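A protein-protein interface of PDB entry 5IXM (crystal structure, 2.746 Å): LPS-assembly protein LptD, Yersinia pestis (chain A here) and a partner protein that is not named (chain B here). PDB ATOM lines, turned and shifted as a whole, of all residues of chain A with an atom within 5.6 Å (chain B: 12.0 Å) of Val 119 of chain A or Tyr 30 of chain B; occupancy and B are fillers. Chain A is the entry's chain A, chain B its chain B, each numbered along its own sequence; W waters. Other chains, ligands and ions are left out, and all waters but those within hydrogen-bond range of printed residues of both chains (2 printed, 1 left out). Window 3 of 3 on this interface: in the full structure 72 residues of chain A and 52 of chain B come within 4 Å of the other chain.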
ATOM      1  N   VAL A 115      12.455  10.945 -21.093  1.00  0.00           N
ATOM      2  CA  VAL A 115      13.011   9.726 -21.658  1.00  0.00           C
ATOM      3  C   VAL A 115      14.099  10.090 -22.661  1.00  0.00           C
ATOM      4  O   VAL A 115      13.814  10.458 -23.800  1.00  0.00           O
ATOM      5  CB  VAL A 115      11.937   8.860 -22.350  1.00  0.00           C
ATOM      6  CG1 VAL A 115      12.562   7.602 -22.932  1.00  0.00           C
ATOM      7  CG2 VAL A 115      10.833   8.501 -21.374  1.00  0.00           C
ATOM      8  N   MET A 116      15.347   9.980 -22.227  1.00  0.00           N
ATOM      9  CA  MET A 116      16.489  10.337 -23.057  1.00  0.00           C
ATOM     10  C   MET A 116      16.962   9.165 -23.907  1.00  0.00           C
ATOM     11  O   MET A 116      17.199   8.064 -23.395  1.00  0.00           O
ATOM     12  CB  MET A 116      17.637  10.840 -22.183  1.00  0.00           C
ATOM     13  CG  MET A 116      18.849  11.320 -22.955  1.00  0.00           C
ATOM     14  SD  MET A 116      20.126  11.918 -21.834  1.00  0.00           S
ATOM     15  CE  MET A 116      20.471  10.420 -20.917  1.00  0.00           C
ATOM     16  N   ASP A 117      17.087   9.417 -25.207  1.00  0.00           N
ATOM     17  CA  ASP A 117      17.588   8.440 -26.169  1.00  0.00           C
ATOM     18  C   ASP A 117      16.773   7.148 -26.133  1.00  0.00           C
ATOM     19  O   ASP A 117      17.308   6.056 -26.324  1.00  0.00           O
ATOM     20  CB  ASP A 117      19.072   8.161 -25.921  1.00  0.00           C
ATOM     21  CG  ASP A 117      19.934   9.401 -26.103  1.00  0.00           C
ATOM     22  OD1 ASP A 117      19.622  10.212 -27.003  1.00  0.00           O
ATOM     23  OD2 ASP A 117      20.921   9.568 -25.353  1.00  0.00           O
ATOM     24  N   GLN A 118      15.478   7.301 -25.864  1.00  0.00           N
ATOM     25  CA  GLN A 118      14.501   6.210 -25.868  1.00  0.00           C
ATOM     26  C   GLN A 118      14.702   5.122 -24.806  1.00  0.00           C
ATOM     27  O   GLN A 118      13.766   4.388 -24.498  1.00  0.00           O
ATOM     28  CB  GLN A 118      14.463   5.549 -27.250  1.00  0.00           C
ATOM     29  CG  GLN A 118      13.946   6.450 -28.355  1.00  0.00           C
ATOM     30  CD  GLN A 118      13.644   5.684 -29.624  1.00  0.00           C
ATOM     31  OE1 GLN A 118      14.184   4.601 -29.850  1.00  0.00           O
ATOM     32  NE2 GLN A 118      12.770   6.236 -30.457  1.00  0.00           N
ATOM     33  N   VAL A 119      15.898   5.019 -24.236  1.00  0.00           N
ATOM     34  CA  VAL A 119      16.183   3.925 -23.313  1.00  0.00           C
ATOM     35  C   VAL A 119      16.481   4.398 -21.893  1.00  0.00           C
ATOM     36  O   VAL A 119      16.448   3.603 -20.953  1.00  0.00           O
ATOM     37  CB  VAL A 119      17.365   3.073 -23.813  1.00  0.00           C
ATOM     38  CG1 VAL A 119      17.010   2.402 -25.127  1.00  0.00           C
ATOM     39  CG2 VAL A 119      18.609   3.929 -23.970  1.00  0.00           C
ATOM     40  N   TRP A 120      16.780   5.684 -21.738  1.00  0.00           N
ATOM     41  CA  TRP A 120      17.047   6.237 -20.414  1.00  0.00           C
ATOM     42  C   TRP A 120      15.809   6.942 -19.873  1.00  0.00           C
ATOM     43  O   TRP A 120      15.105   7.623 -20.610  1.00  0.00           O
ATOM     44  CB  TRP A 120      18.248   7.182 -20.462  1.00  0.00           C
ATOM     45  CG  TRP A 120      19.478   6.495 -20.971  1.00  0.00           C
ATOM     46  CD1 TRP A 120      20.027   6.609 -22.215  1.00  0.00           C
ATOM     47  CD2 TRP A 120      20.291   5.557 -20.258  1.00  0.00           C
ATOM     48  NE1 TRP A 120      21.140   5.811 -22.316  1.00  0.00           N
ATOM     49  CE2 TRP A 120      21.323   5.154 -21.127  1.00  0.00           C
ATOM     50  CE3 TRP A 120      20.250   5.022 -18.966  1.00  0.00           C
ATOM     51  CZ2 TRP A 120      22.308   4.241 -20.746  1.00  0.00           C
ATOM     52  CZ3 TRP A 120      21.227   4.114 -18.590  1.00  0.00           C
ATOM     53  CH2 TRP A 120      22.241   3.734 -19.477  1.00  0.00           C
ATOM     54  N   ARG A 121      15.530   6.749 -18.588  1.00  0.00           N
ATOM     55  CA  ARG A 121      14.299   7.249 -17.989  1.00  0.00           C
ATOM     56  C   ARG A 121      14.584   7.980 -16.680  1.00  0.00           C
ATOM     57  O   ARG A 121      15.116   7.392 -15.734  1.00  0.00           O
ATOM     58  CB  ARG A 121      13.311   6.100 -17.752  1.00  0.00           C
ATOM     59  CG  ARG A 121      13.123   5.186 -18.952  1.00  0.00           C
ATOM     60  CD  ARG A 121      12.021   4.163 -18.726  1.00  0.00           C
ATOM     61  NE  ARG A 121      10.695   4.770 -18.676  1.00  0.00           N
ATOM     62  CZ  ARG A 121       9.991   5.117 -19.749  1.00  0.00           C
ATOM     63  NH1 ARG A 121      10.490   4.928 -20.966  1.00  0.00           N
ATOM     64  NH2 ARG A 121       8.790   5.660 -19.608  1.00  0.00           N
ATOM     65  N   GLY A 157      16.405   5.048 -14.567  1.00  0.00           N
ATOM     66  CA  GLY A 157      16.352   3.678 -15.035  1.00  0.00           C
ATOM     67  C   GLY A 157      16.629   3.468 -16.508  1.00  0.00           C
ATOM     68  O   GLY A 157      16.585   4.396 -17.310  1.00  0.00           O
ATOM     69  N   TYR A 158      16.919   2.220 -16.858  1.00  0.00           N
ATOM     70  CA  TYR A 158      17.123   1.825 -18.239  1.00  0.00           C
ATOM     71  C   TYR A 158      15.971   0.935 -18.685  1.00  0.00           C
ATOM     72  O   TYR A 158      15.390   0.217 -17.872  1.00  0.00           O
ATOM     73  CB  TYR A 158      18.466   1.105 -18.390  1.00  0.00           C
ATOM     74  CG  TYR A 158      18.761   0.601 -19.786  1.00  0.00           C
ATOM     75  CD1 TYR A 158      19.342   1.431 -20.737  1.00  0.00           C
ATOM     76  CD2 TYR A 158      18.472  -0.711 -20.149  1.00  0.00           C
ATOM     77  CE1 TYR A 158      19.616   0.976 -22.015  1.00  0.00           C
ATOM     78  CE2 TYR A 158      18.743  -1.176 -21.427  1.00  0.00           C
ATOM     79  CZ  TYR A 158      19.315  -0.328 -22.356  1.00  0.00           C
ATOM     80  OH  TYR A 158      19.590  -0.781 -23.627  1.00  0.00           O
ATOM     81  N   ALA A 159      15.635   0.982 -19.969  1.00  0.00           N
ATOM     82  CA  ALA A 159      14.564   0.144 -20.496  1.00  0.00           C
ATOM     83  C   ALA A 159      14.668  -0.054 -22.000  1.00  0.00           C
ATOM     84  O   ALA A 159      14.846   0.904 -22.750  1.00  0.00           O
ATOM     85  CB  ALA A 159      13.212   0.741 -20.152  1.00  0.00           C
ATOM     86  N   ASN A 160      14.558  -1.304 -22.435  1.00  0.00           N
ATOM     87  CA  ASN A 160      14.398  -1.597 -23.852  1.00  0.00           C
ATOM     88  C   ASN A 160      13.249  -2.579 -24.040  1.00  0.00           C
ATOM     89  O   ASN A 160      12.431  -2.763 -23.139  1.00  0.00           O
ATOM     90  CB  ASN A 160      15.695  -2.139 -24.472  1.00  0.00           C
ATOM     91  CG  ASN A 160      16.238  -3.364 -23.752  1.00  0.00           C
ATOM     92  OD1 ASN A 160      15.487  -4.222 -23.284  1.00  0.00           O
ATOM     93  ND2 ASN A 160      17.561  -3.454 -23.672  1.00  0.00           N
ATOM     94  N   GLU A 161      13.194  -3.213 -25.203  1.00  0.00           N
ATOM     95  CA  GLU A 161      12.098  -4.118 -25.532  1.00  0.00           C
ATOM     96  C   GLU A 161      12.010  -5.365 -24.647  1.00  0.00           C
ATOM     97  O   GLU A 161      10.919  -5.876 -24.405  1.00  0.00           O
ATOM     98  CB  GLU A 161      12.207  -4.524 -27.011  1.00  0.00           C
ATOM     99  CG  GLU A 161      13.395  -5.425 -27.331  1.00  0.00           C
ATOM    100  CD  GLU A 161      14.691  -4.634 -27.488  1.00  0.00           C
ATOM    101  OE1 GLU A 161      14.662  -3.398 -27.286  1.00  0.00           O
ATOM    102  OE2 GLU A 161      15.734  -5.243 -27.805  1.00  0.00           O
ATOM    103  N   LEU B  24       3.068  -0.009 -35.367  1.00  0.00           N
ATOM    104  CA  LEU B  24       2.877   0.579 -34.050  1.00  0.00           C
ATOM    105  C   LEU B  24       3.978   1.574 -33.732  1.00  0.00           C
ATOM    106  O   LEU B  24       5.113   1.182 -33.458  1.00  0.00           O
ATOM    107  CB  LEU B  24       2.825  -0.510 -32.978  1.00  0.00           C
ATOM    108  CG  LEU B  24       2.576  -0.028 -31.550  1.00  0.00           C
ATOM    109  CD1 LEU B  24       1.240   0.683 -31.469  1.00  0.00           C
ATOM    110  CD2 LEU B  24       2.624  -1.193 -30.575  1.00  0.00           C
ATOM    111  N   GLU B  25       3.652   2.859 -33.770  1.00  0.00           N
ATOM    112  CA  GLU B  25       4.642   3.871 -33.431  1.00  0.00           C
ATOM    113  C   GLU B  25       4.272   4.535 -32.116  1.00  0.00           C
ATOM    114  O   GLU B  25       3.095   4.681 -31.799  1.00  0.00           O
ATOM    115  CB  GLU B  25       4.773   4.912 -34.541  1.00  0.00           C
ATOM    116  CG  GLU B  25       5.348   4.355 -35.831  1.00  0.00           C
ATOM    117  CD  GLU B  25       5.398   5.383 -36.942  1.00  0.00           C
ATOM    118  OE1 GLU B  25       4.848   6.488 -36.756  1.00  0.00           O
ATOM    119  OE2 GLU B  25       5.982   5.083 -38.004  1.00  0.00           O
ATOM    120  N   SER B  26       5.282   4.930 -31.351  1.00  0.00           N
ATOM    121  CA  SER B  26       5.043   5.512 -30.041  1.00  0.00           C
ATOM    122  C   SER B  26       6.163   6.468 -29.662  1.00  0.00           C
ATOM    123  O   SER B  26       7.325   6.250 -30.004  1.00  0.00           O
ATOM    124  CB  SER B  26       4.904   4.412 -28.985  1.00  0.00           C
ATOM    125  OG  SER B  26       4.721   4.964 -27.693  1.00  0.00           O
ATOM    126  N   SER B  27       5.796   7.533 -28.958  1.00  0.00           N
ATOM    127  CA  SER B  27       6.762   8.465 -28.398  1.00  0.00           C
ATOM    128  C   SER B  27       7.652   7.759 -27.384  1.00  0.00           C
ATOM    129  O   SER B  27       8.793   8.159 -27.153  1.00  0.00           O
ATOM    130  CB  SER B  27       6.046   9.647 -27.745  1.00  0.00           C
ATOM    131  OG  SER B  27       5.120   9.200 -26.769  1.00  0.00           O
ATOM    132  N   ASP B  28       7.114   6.705 -26.780  1.00  0.00           N
ATOM    133  CA  ASP B  28       7.815   5.968 -25.739  1.00  0.00           C
ATOM    134  C   ASP B  28       7.725   4.461 -25.997  1.00  0.00           C
ATOM    135  O   ASP B  28       6.974   3.760 -25.320  1.00  0.00           O
ATOM    136  CB  ASP B  28       7.220   6.320 -24.374  1.00  0.00           C
ATOM    137  CG  ASP B  28       8.166   6.044 -23.227  1.00  0.00           C
ATOM    138  OD1 ASP B  28       9.174   5.337 -23.432  1.00  0.00           O
ATOM    139  OD2 ASP B  28       7.893   6.541 -22.113  1.00  0.00           O
ATOM    140  N   PRO B  29       8.493   3.963 -26.983  1.00  0.00           N
ATOM    141  CA  PRO B  29       8.429   2.567 -27.439  1.00  0.00           C
ATOM    142  C   PRO B  29       8.781   1.541 -26.366  1.00  0.00           C
ATOM    143  O   PRO B  29       8.310   0.405 -26.432  1.00  0.00           O
ATOM    144  CB  PRO B  29       9.461   2.521 -28.573  1.00  0.00           C
ATOM    145  CG  PRO B  29       9.585   3.926 -29.030  1.00  0.00           C
ATOM    146  CD  PRO B  29       9.442   4.749 -27.790  1.00  0.00           C
ATOM    147  N   TYR B  30       9.594   1.938 -25.395  1.00  0.00           N
ATOM    148  CA  TYR B  30      10.073   1.012 -24.380  1.00  0.00           C
ATOM    149  C   TYR B  30       9.430   1.291 -23.027  1.00  0.00           C
ATOM    150  O   TYR B  30       9.808   0.705 -22.014  1.00  0.00           O
ATOM    151  CB  TYR B  30      11.596   1.101 -24.270  1.00  0.00           C
ATOM    152  CG  TYR B  30      12.315   0.836 -25.575  1.00  0.00           C
ATOM    153  CD1 TYR B  30      11.850  -0.127 -26.465  1.00  0.00           C
ATOM    154  CD2 TYR B  30      13.444   1.564 -25.929  1.00  0.00           C
ATOM    155  CE1 TYR B  30      12.501  -0.368 -27.661  1.00  0.00           C
ATOM    156  CE2 TYR B  30      14.100   1.331 -27.125  1.00  0.00           C
ATOM    157  CZ  TYR B  30      13.623   0.365 -27.987  1.00  0.00           C
ATOM    158  OH  TYR B  30      14.272   0.128 -29.178  1.00  0.00           O
ATOM    159  N   GLY B  31       8.454   2.194 -23.021  1.00  0.00           N
ATOM    160  CA  GLY B  31       7.730   2.529 -21.809  1.00  0.00           C
ATOM    161  C   GLY B  31       6.685   1.481 -21.472  1.00  0.00           C
ATOM    162  O   GLY B  31       6.326   0.666 -22.321  1.00  0.00           O
ATOM    163  N   PRO B  32       6.191   1.498 -20.226  1.00  0.00           N
ATOM    164  CA  PRO B  32       5.206   0.520 -19.746  1.00  0.00           C
ATOM    165  C   PRO B  32       3.882   0.560 -20.518  1.00  0.00           C
ATOM    166  O   PRO B  32       3.285  -0.493 -20.764  1.00  0.00           O
ATOM    167  CB  PRO B  32       5.006   0.915 -18.277  1.00  0.00           C
ATOM    168  CG  PRO B  32       5.498   2.325 -18.179  1.00  0.00           C
ATOM    169  CD  PRO B  32       6.607   2.433 -19.168  1.00  0.00           C
ATOM    170  N   LEU B  33       3.432   1.753 -20.895  1.00  0.00           N
ATOM    171  CA  LEU B  33       2.198   1.891 -21.661  1.00  0.00           C
ATOM    172  C   LEU B  33       2.300   1.149 -22.991  1.00  0.00           C
ATOM    173  O   LEU B  33       1.388   0.412 -23.375  1.00  0.00           O
ATOM    174  CB  LEU B  33       1.865   3.366 -21.898  1.00  0.00           C
ATOM    175  CG  LEU B  33       0.675   3.656 -22.819  1.00  0.00           C
ATOM    176  CD1 LEU B  33      -0.592   2.973 -22.325  1.00  0.00           C
ATOM    177  CD2 LEU B  33       0.458   5.156 -22.952  1.00  0.00           C
ATOM    178  N   ALA B  34       3.420   1.340 -23.683  1.00  0.00           N
ATOM    179  CA  ALA B  34       3.658   0.669 -24.956  1.00  0.00           C
ATOM    180  C   ALA B  34       3.688  -0.846 -24.781  1.00  0.00           C
ATOM    181  O   ALA B  34       3.235  -1.595 -25.655  1.00  0.00           O
ATOM    182  CB  ALA B  34       4.957   1.154 -25.577  1.00  0.00           C
ATOM    183  N   ARG B  35       4.209  -1.298 -23.645  1.00  0.00           N
ATOM    184  CA  ARG B  35       4.236  -2.724 -23.351  1.00  0.00           C
ATOM    185  C   ARG B  35       2.818  -3.257 -23.175  1.00  0.00           C
ATOM    186  O   ARG B  35       2.478  -4.311 -23.709  1.00  0.00           O
ATOM    187  CB  ARG B  35       5.084  -3.013 -22.107  1.00  0.00           C
ATOM    188  CG  ARG B  35       4.901  -4.420 -21.545  1.00  0.00           C
ATOM    189  CD  ARG B  35       6.040  -4.830 -20.619  1.00  0.00           C
ATOM    190  NE  ARG B  35       7.160  -5.419 -21.349  1.00  0.00           N
ATOM    191  CZ  ARG B  35       8.255  -4.756 -21.706  1.00  0.00           C
ATOM    192  NH1 ARG B  35       8.381  -3.473 -21.399  1.00  0.00           N
ATOM    193  NH2 ARG B  35       9.222  -5.377 -22.368  1.00  0.00           N
ATOM    194  N   SER B  36       1.995  -2.531 -22.423  1.00  0.00           N
ATOM    195  CA  SER B  36       0.605  -2.933 -22.227  1.00  0.00           C
ATOM    196  C   SER B  36      -0.144  -2.997 -23.556  1.00  0.00           C
ATOM    197  O   SER B  36      -0.889  -3.948 -23.819  1.00  0.00           O
ATOM    198  CB  SER B  36      -0.106  -1.975 -21.267  1.00  0.00           C
ATOM    199  OG  SER B  36       0.470  -2.016 -19.974  1.00  0.00           O
ATOM    200  N   ILE B  37       0.069  -1.987 -24.396  1.00  0.00           N
ATOM    201  CA  ILE B  37      -0.571  -1.933 -25.705  1.00  0.00           C
ATOM    202  C   ILE B  37      -0.139  -3.114 -26.571  1.00  0.00           C
ATOM    203  O   ILE B  37      -0.962  -3.717 -27.264  1.00  0.00           O
ATOM    204  CB  ILE B  37      -0.267  -0.600 -26.421  1.00  0.00           C
ATOM    205  CG1 ILE B  37      -0.885   0.557 -25.633  1.00  0.00           C
ATOM    206  CG2 ILE B  37      -0.818  -0.607 -27.841  1.00  0.00           C
ATOM    207  CD1 ILE B  37      -0.601   1.920 -26.210  1.00  0.00           C
ATOM    208  N   ARG B  38       1.146  -3.454 -26.520  1.00  0.00           N
ATOM    209  CA  ARG B  38       1.644  -4.617 -27.250  1.00  0.00           C
ATOM    210  C   ARG B  38       1.033  -5.922 -26.748  1.00  0.00           C
ATOM    211  O   ARG B  38       0.646  -6.777 -27.545  1.00  0.00           O
ATOM    212  CB  ARG B  38       3.168  -4.695 -27.182  1.00  0.00           C
ATOM    213  CG  ARG B  38       3.849  -3.775 -28.166  1.00  0.00           C
ATOM    214  CD  ARG B  38       5.340  -4.020 -28.230  1.00  0.00           C
ATOM    215  NE  ARG B  38       5.876  -3.538 -29.498  1.00  0.00           N
ATOM    216  CZ  ARG B  38       6.364  -2.317 -29.687  1.00  0.00           C
ATOM    217  NH1 ARG B  38       6.383  -1.447 -28.685  1.00  0.00           N
ATOM    218  NH2 ARG B  38       6.825  -1.967 -30.880  1.00  0.00           N
ATOM    219  N   GLN B  39       0.957  -6.073 -25.430  1.00  0.00           N
ATOM    220  CA  GLN B  39       0.369  -7.266 -24.831  1.00  0.00           C
ATOM    221  C   GLN B  39      -1.081  -7.424 -25.268  1.00  0.00           C
ATOM    222  O   GLN B  39      -1.529  -8.526 -25.590  1.00  0.00           O
ATOM    223  CB  GLN B  39       0.448  -7.196 -23.305  1.00  0.00           C
ATOM    224  CG  GLN B  39       1.854  -7.290 -22.741  1.00  0.00           C
ATOM    225  CD  GLN B  39       1.884  -7.117 -21.236  1.00  0.00           C
ATOM    226  OE1 GLN B  39       0.861  -6.827 -20.613  1.00  0.00           O
ATOM    227  NE2 GLN B  39       3.063  -7.284 -20.642  1.00  0.00           N
ATOM    228  N   ILE B  48       2.217  -7.465 -35.046  1.00  0.00           N
ATOM    229  CA  ILE B  48       2.871  -6.158 -35.026  1.00  0.00           C
ATOM    230  C   ILE B  48       4.194  -6.203 -35.781  1.00  0.00           C
ATOM    231  O   ILE B  48       5.183  -6.740 -35.278  1.00  0.00           O
ATOM    232  CB  ILE B  48       3.126  -5.672 -33.591  1.00  0.00           C
ATOM    233  CG1 ILE B  48       1.864  -5.823 -32.740  1.00  0.00           C
ATOM    234  CG2 ILE B  48       3.627  -4.233 -33.599  1.00  0.00           C
ATOM    235  CD1 ILE B  48       2.069  -5.469 -31.283  1.00  0.00           C
ATOM    236  N   ASP B  50       7.441  -4.660 -38.491  1.00  0.00           N
ATOM    237  CA  ASP B  50       8.530  -3.693 -38.562  1.00  0.00           C
ATOM    238  C   ASP B  50       8.701  -2.921 -39.874  1.00  0.00           C
ATOM    239  O   ASP B  50       9.780  -2.391 -40.128  1.00  0.00           O
ATOM    240  CB  ASP B  50       9.832  -4.446 -38.310  1.00  0.00           C
ATOM    241  CG  ASP B  50      10.081  -5.526 -39.363  1.00  0.00           C
ATOM    242  OD1 ASP B  50       9.105  -6.184 -39.791  1.00  0.00           O
ATOM    243  OD2 ASP B  50      11.242  -5.697 -39.787  1.00  0.00           O
ATOM    244  N   ILE B  62       0.795   6.228 -31.016  1.00  0.00           N
ATOM    245  CA  ILE B  62       0.556   6.777 -29.694  1.00  0.00           C
ATOM    246  C   ILE B  62       1.298   8.104 -29.612  1.00  0.00           C
ATOM    247  O   ILE B  62       2.530   8.142 -29.584  1.00  0.00           O
ATOM    248  CB  ILE B  62       1.007   5.820 -28.570  1.00  0.00           C
ATOM    249  CG1 ILE B  62       0.005   4.673 -28.409  1.00  0.00           C
ATOM    250  CG2 ILE B  62       1.118   6.557 -27.249  1.00  0.00           C
ATOM    251  CD1 ILE B  62       0.126   3.577 -29.440  1.00  0.00           C
ATOM    252  N   ILE B  63       0.537   9.194 -29.600  1.00  0.00           N
ATOM    253  CA  ILE B  63       1.113  10.534 -29.595  1.00  0.00           C
ATOM    254  C   ILE B  63       1.809  10.805 -28.272  1.00  0.00           C
ATOM    255  O   ILE B  63       2.967  11.219 -28.237  1.00  0.00           O
ATOM    256  CB  ILE B  63       0.044  11.611 -29.838  1.00  0.00           C
ATOM    257  CG1 ILE B  63      -0.564  11.452 -31.231  1.00  0.00           C
ATOM    258  CG2 ILE B  63       0.639  13.000 -29.666  1.00  0.00           C
ATOM    259  CD1 ILE B  63      -1.662  12.450 -31.526  1.00  0.00           C
ATOM    260  N   GLY B  64       1.093  10.559 -27.183  1.00  0.00           N
ATOM    261  CA  GLY B  64       1.643  10.758 -25.859  1.00  0.00           C
ATOM    262  C   GLY B  64       0.657  10.376 -24.780  1.00  0.00           C
ATOM    263  O   GLY B  64      -0.448   9.918 -25.068  1.00  0.00           O
ATOM    264  N   SER B  65       1.065  10.569 -23.530  1.00  0.00           N
ATOM    265  CA  SER B  65       0.221  10.252 -22.389  1.00  0.00           C
ATOM    266  C   SER B  65       0.569  11.150 -21.209  1.00  0.00           C
ATOM    267  O   SER B  65       1.713  11.582 -21.066  1.00  0.00           O
ATOM    268  CB  SER B  65       0.373   8.780 -22.002  1.00  0.00           C
ATOM    269  OG  SER B  65       1.680   8.509 -21.524  1.00  0.00           O
ATOM    270  N   GLN B 130      -0.139   0.939 -12.891  1.00  0.00           N
ATOM    271  CA  GLN B 130       0.050  -0.235 -13.729  1.00  0.00           C
ATOM    272  C   GLN B 130      -1.290  -0.653 -14.308  1.00  0.00           C
ATOM    273  O   GLN B 130      -1.477  -0.659 -15.532  1.00  0.00           O
ATOM    274  CB  GLN B 130       0.663  -1.375 -12.909  1.00  0.00           C
ATOM    275  CG  GLN B 130       0.745  -2.724 -13.610  1.00  0.00           C
ATOM    276  CD  GLN B 130       1.561  -2.689 -14.880  1.00  0.00           C
ATOM    277  OE1 GLN B 130       2.451  -1.853 -15.035  1.00  0.00           O
ATOM    278  NE2 GLN B 130       1.267  -3.604 -15.800  1.00  0.00           N
ATOM    279  N   ARG B 133      -2.748   1.700 -16.881  1.00  0.00           N
ATOM    280  CA  ARG B 133      -2.109   1.586 -18.179  1.00  0.00           C
ATOM    281  C   ARG B 133      -2.734   0.426 -18.934  1.00  0.00           C
ATOM    282  O   ARG B 133      -3.192   0.589 -20.074  1.00  0.00           O
ATOM    283  CB  ARG B 133      -0.596   1.412 -18.036  1.00  0.00           C
ATOM    284  CG  ARG B 133       0.138   2.728 -17.805  1.00  0.00           C
ATOM    285  CD  ARG B 133       1.651   2.563 -17.786  1.00  0.00           C
ATOM    286  NE  ARG B 133       2.126   1.919 -16.566  1.00  0.00           N
ATOM    287  CZ  ARG B 133       2.527   2.582 -15.487  1.00  0.00           C
ATOM    288  NH1 ARG B 133       2.520   3.908 -15.485  1.00  0.00           N
ATOM    289  NH2 ARG B 133       2.943   1.922 -14.416  1.00  0.00           N
HETATM  290  O   HOH W   1       9.774   6.596 -31.668  1.00  0.00           O
HETATM  291  O   HOH W   2      10.961  -2.871 -20.992  1.00  0.00           O
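Among the printed residues, pairs that only touch across the chains: Val 115 of chain A with Asp 28 of chain B (3.6 Å), Gln 118 of chain A with Tyr 30 of chain B (3.2 Å), Val 119 of chain A with Tyr 30 of chain B (3.7 Å), Arg 121 of chain A with Gly 31 of chain B (3.8 Å), Arg 121 of chain A with Pro 32 of chain B (3.9 Å), Ala 159 of chain A with Tyr 30 of chain B (3.5 Å), Asn 160 of chain A with Tyr 30 of chain B (3.6 Å) and Glu 161 of chain A with Tyr 30 of chain B (3.6 Å).
NH2 of Arg 121 of chain A lies within salt-bridge range of OD2 of Asp 28 of chain B. The guanidinium group (NH2) of Arg 35 of chain B lies within hydrogen-bond range of the backbone carbonyl oxygen (O) of Glu 161 of chain A.
N of Ala 159 of chain A is in hydrogen-bond range of O of Val 119 of chain A (2.9 Å). The backbone NH (N) of Arg 121 of chain A is in hydrogen-bond range of the backbone carbonyl oxygen (O) of Gly 157 of chain A (2.9 Å). O of Pro 32 of chain B lies within hydrogen-bond range of OG of Ser 36 of chain B (3.3 Å). The side-chain hydroxyl of Ser 26 of chain B lies close to the backbone NH of Asp 28 of chain B (3.1 Å). The side-chain hydroxyl of Tyr 158 of chain A sits at hydrogen-bond distance from the side-chain amide nitrogen of Asn 160 of chain A (3.4 Å). The side-chain carboxylate (OD1) of Asp 28 of chain B is in hydrogen-bond range of the backbone NH (N) of Gly 31 of chain B.
Water W2 bridges O of Asn 160 of chain A (2.6 Å) and NH1 of Arg 35 of chain B (2.7 Å). Water W1 lies within hydrogen-bond range of the backbone carbonyl oxygen (O) of Ser 26 of chain B (3.0 Å) and the side-chain amide nitrogen (NE2) of Gln 118 of chain A (3.3 Å).
Of chain B, only Tyr 30 (3.7 Å) comes within 4 Å of Val 119 of chain A. Printed residues of chain A within 4 Å of Tyr 30 of chain B: Gln 118, Val 119, Ala 159, Asn 160 and Glu 161. Of chain B, only Asp 28 (3.6 Å) comes within 4 Å of Val 115 of chain A. No residue of chain B comes within 4 Å of Asp 117 of chain A. No residue of chain B comes within 4 Å of Trp 120 of chain A. No residue of chain B comes within 4 Å of Gly 157 of chain A. No residue of chain B comes within 4 Å of Tyr 158 of chain A. Ala 159 of chain A touches one residue of chain B. Asn 160 of chain A touches just one residue of chain B: Tyr 30. Of the printed residues of chain A, Arg 35 of chain B touches Glu 161 (2.7 Å). Of the printed residues of chain A, Asp 28 of chain B touches Val 115 (3.6 Å) and Arg 121 (2.8 Å). Leu 24 of chain B touches none of the printed residues of chain A. Ile 63 of chain B touches none of the printed residues of chain A. The nearest residue of chain B that does not touch Val 119 of chain A is Asp 28 of chain B (6.8 Å).
Hydrophobic or aromatic side chains of chain B that line the printed part of chain A: Tyr 30 and Pro 32. Among the printed residues, 10 pairs touch across the chains. Among the printed residues, Asp or Glu carboxylates within 4 Å of a Lys or Arg side-chain nitrogen of the other chain: Arg 121 of chain A with Asp 28 of chain B (2.8 Å).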
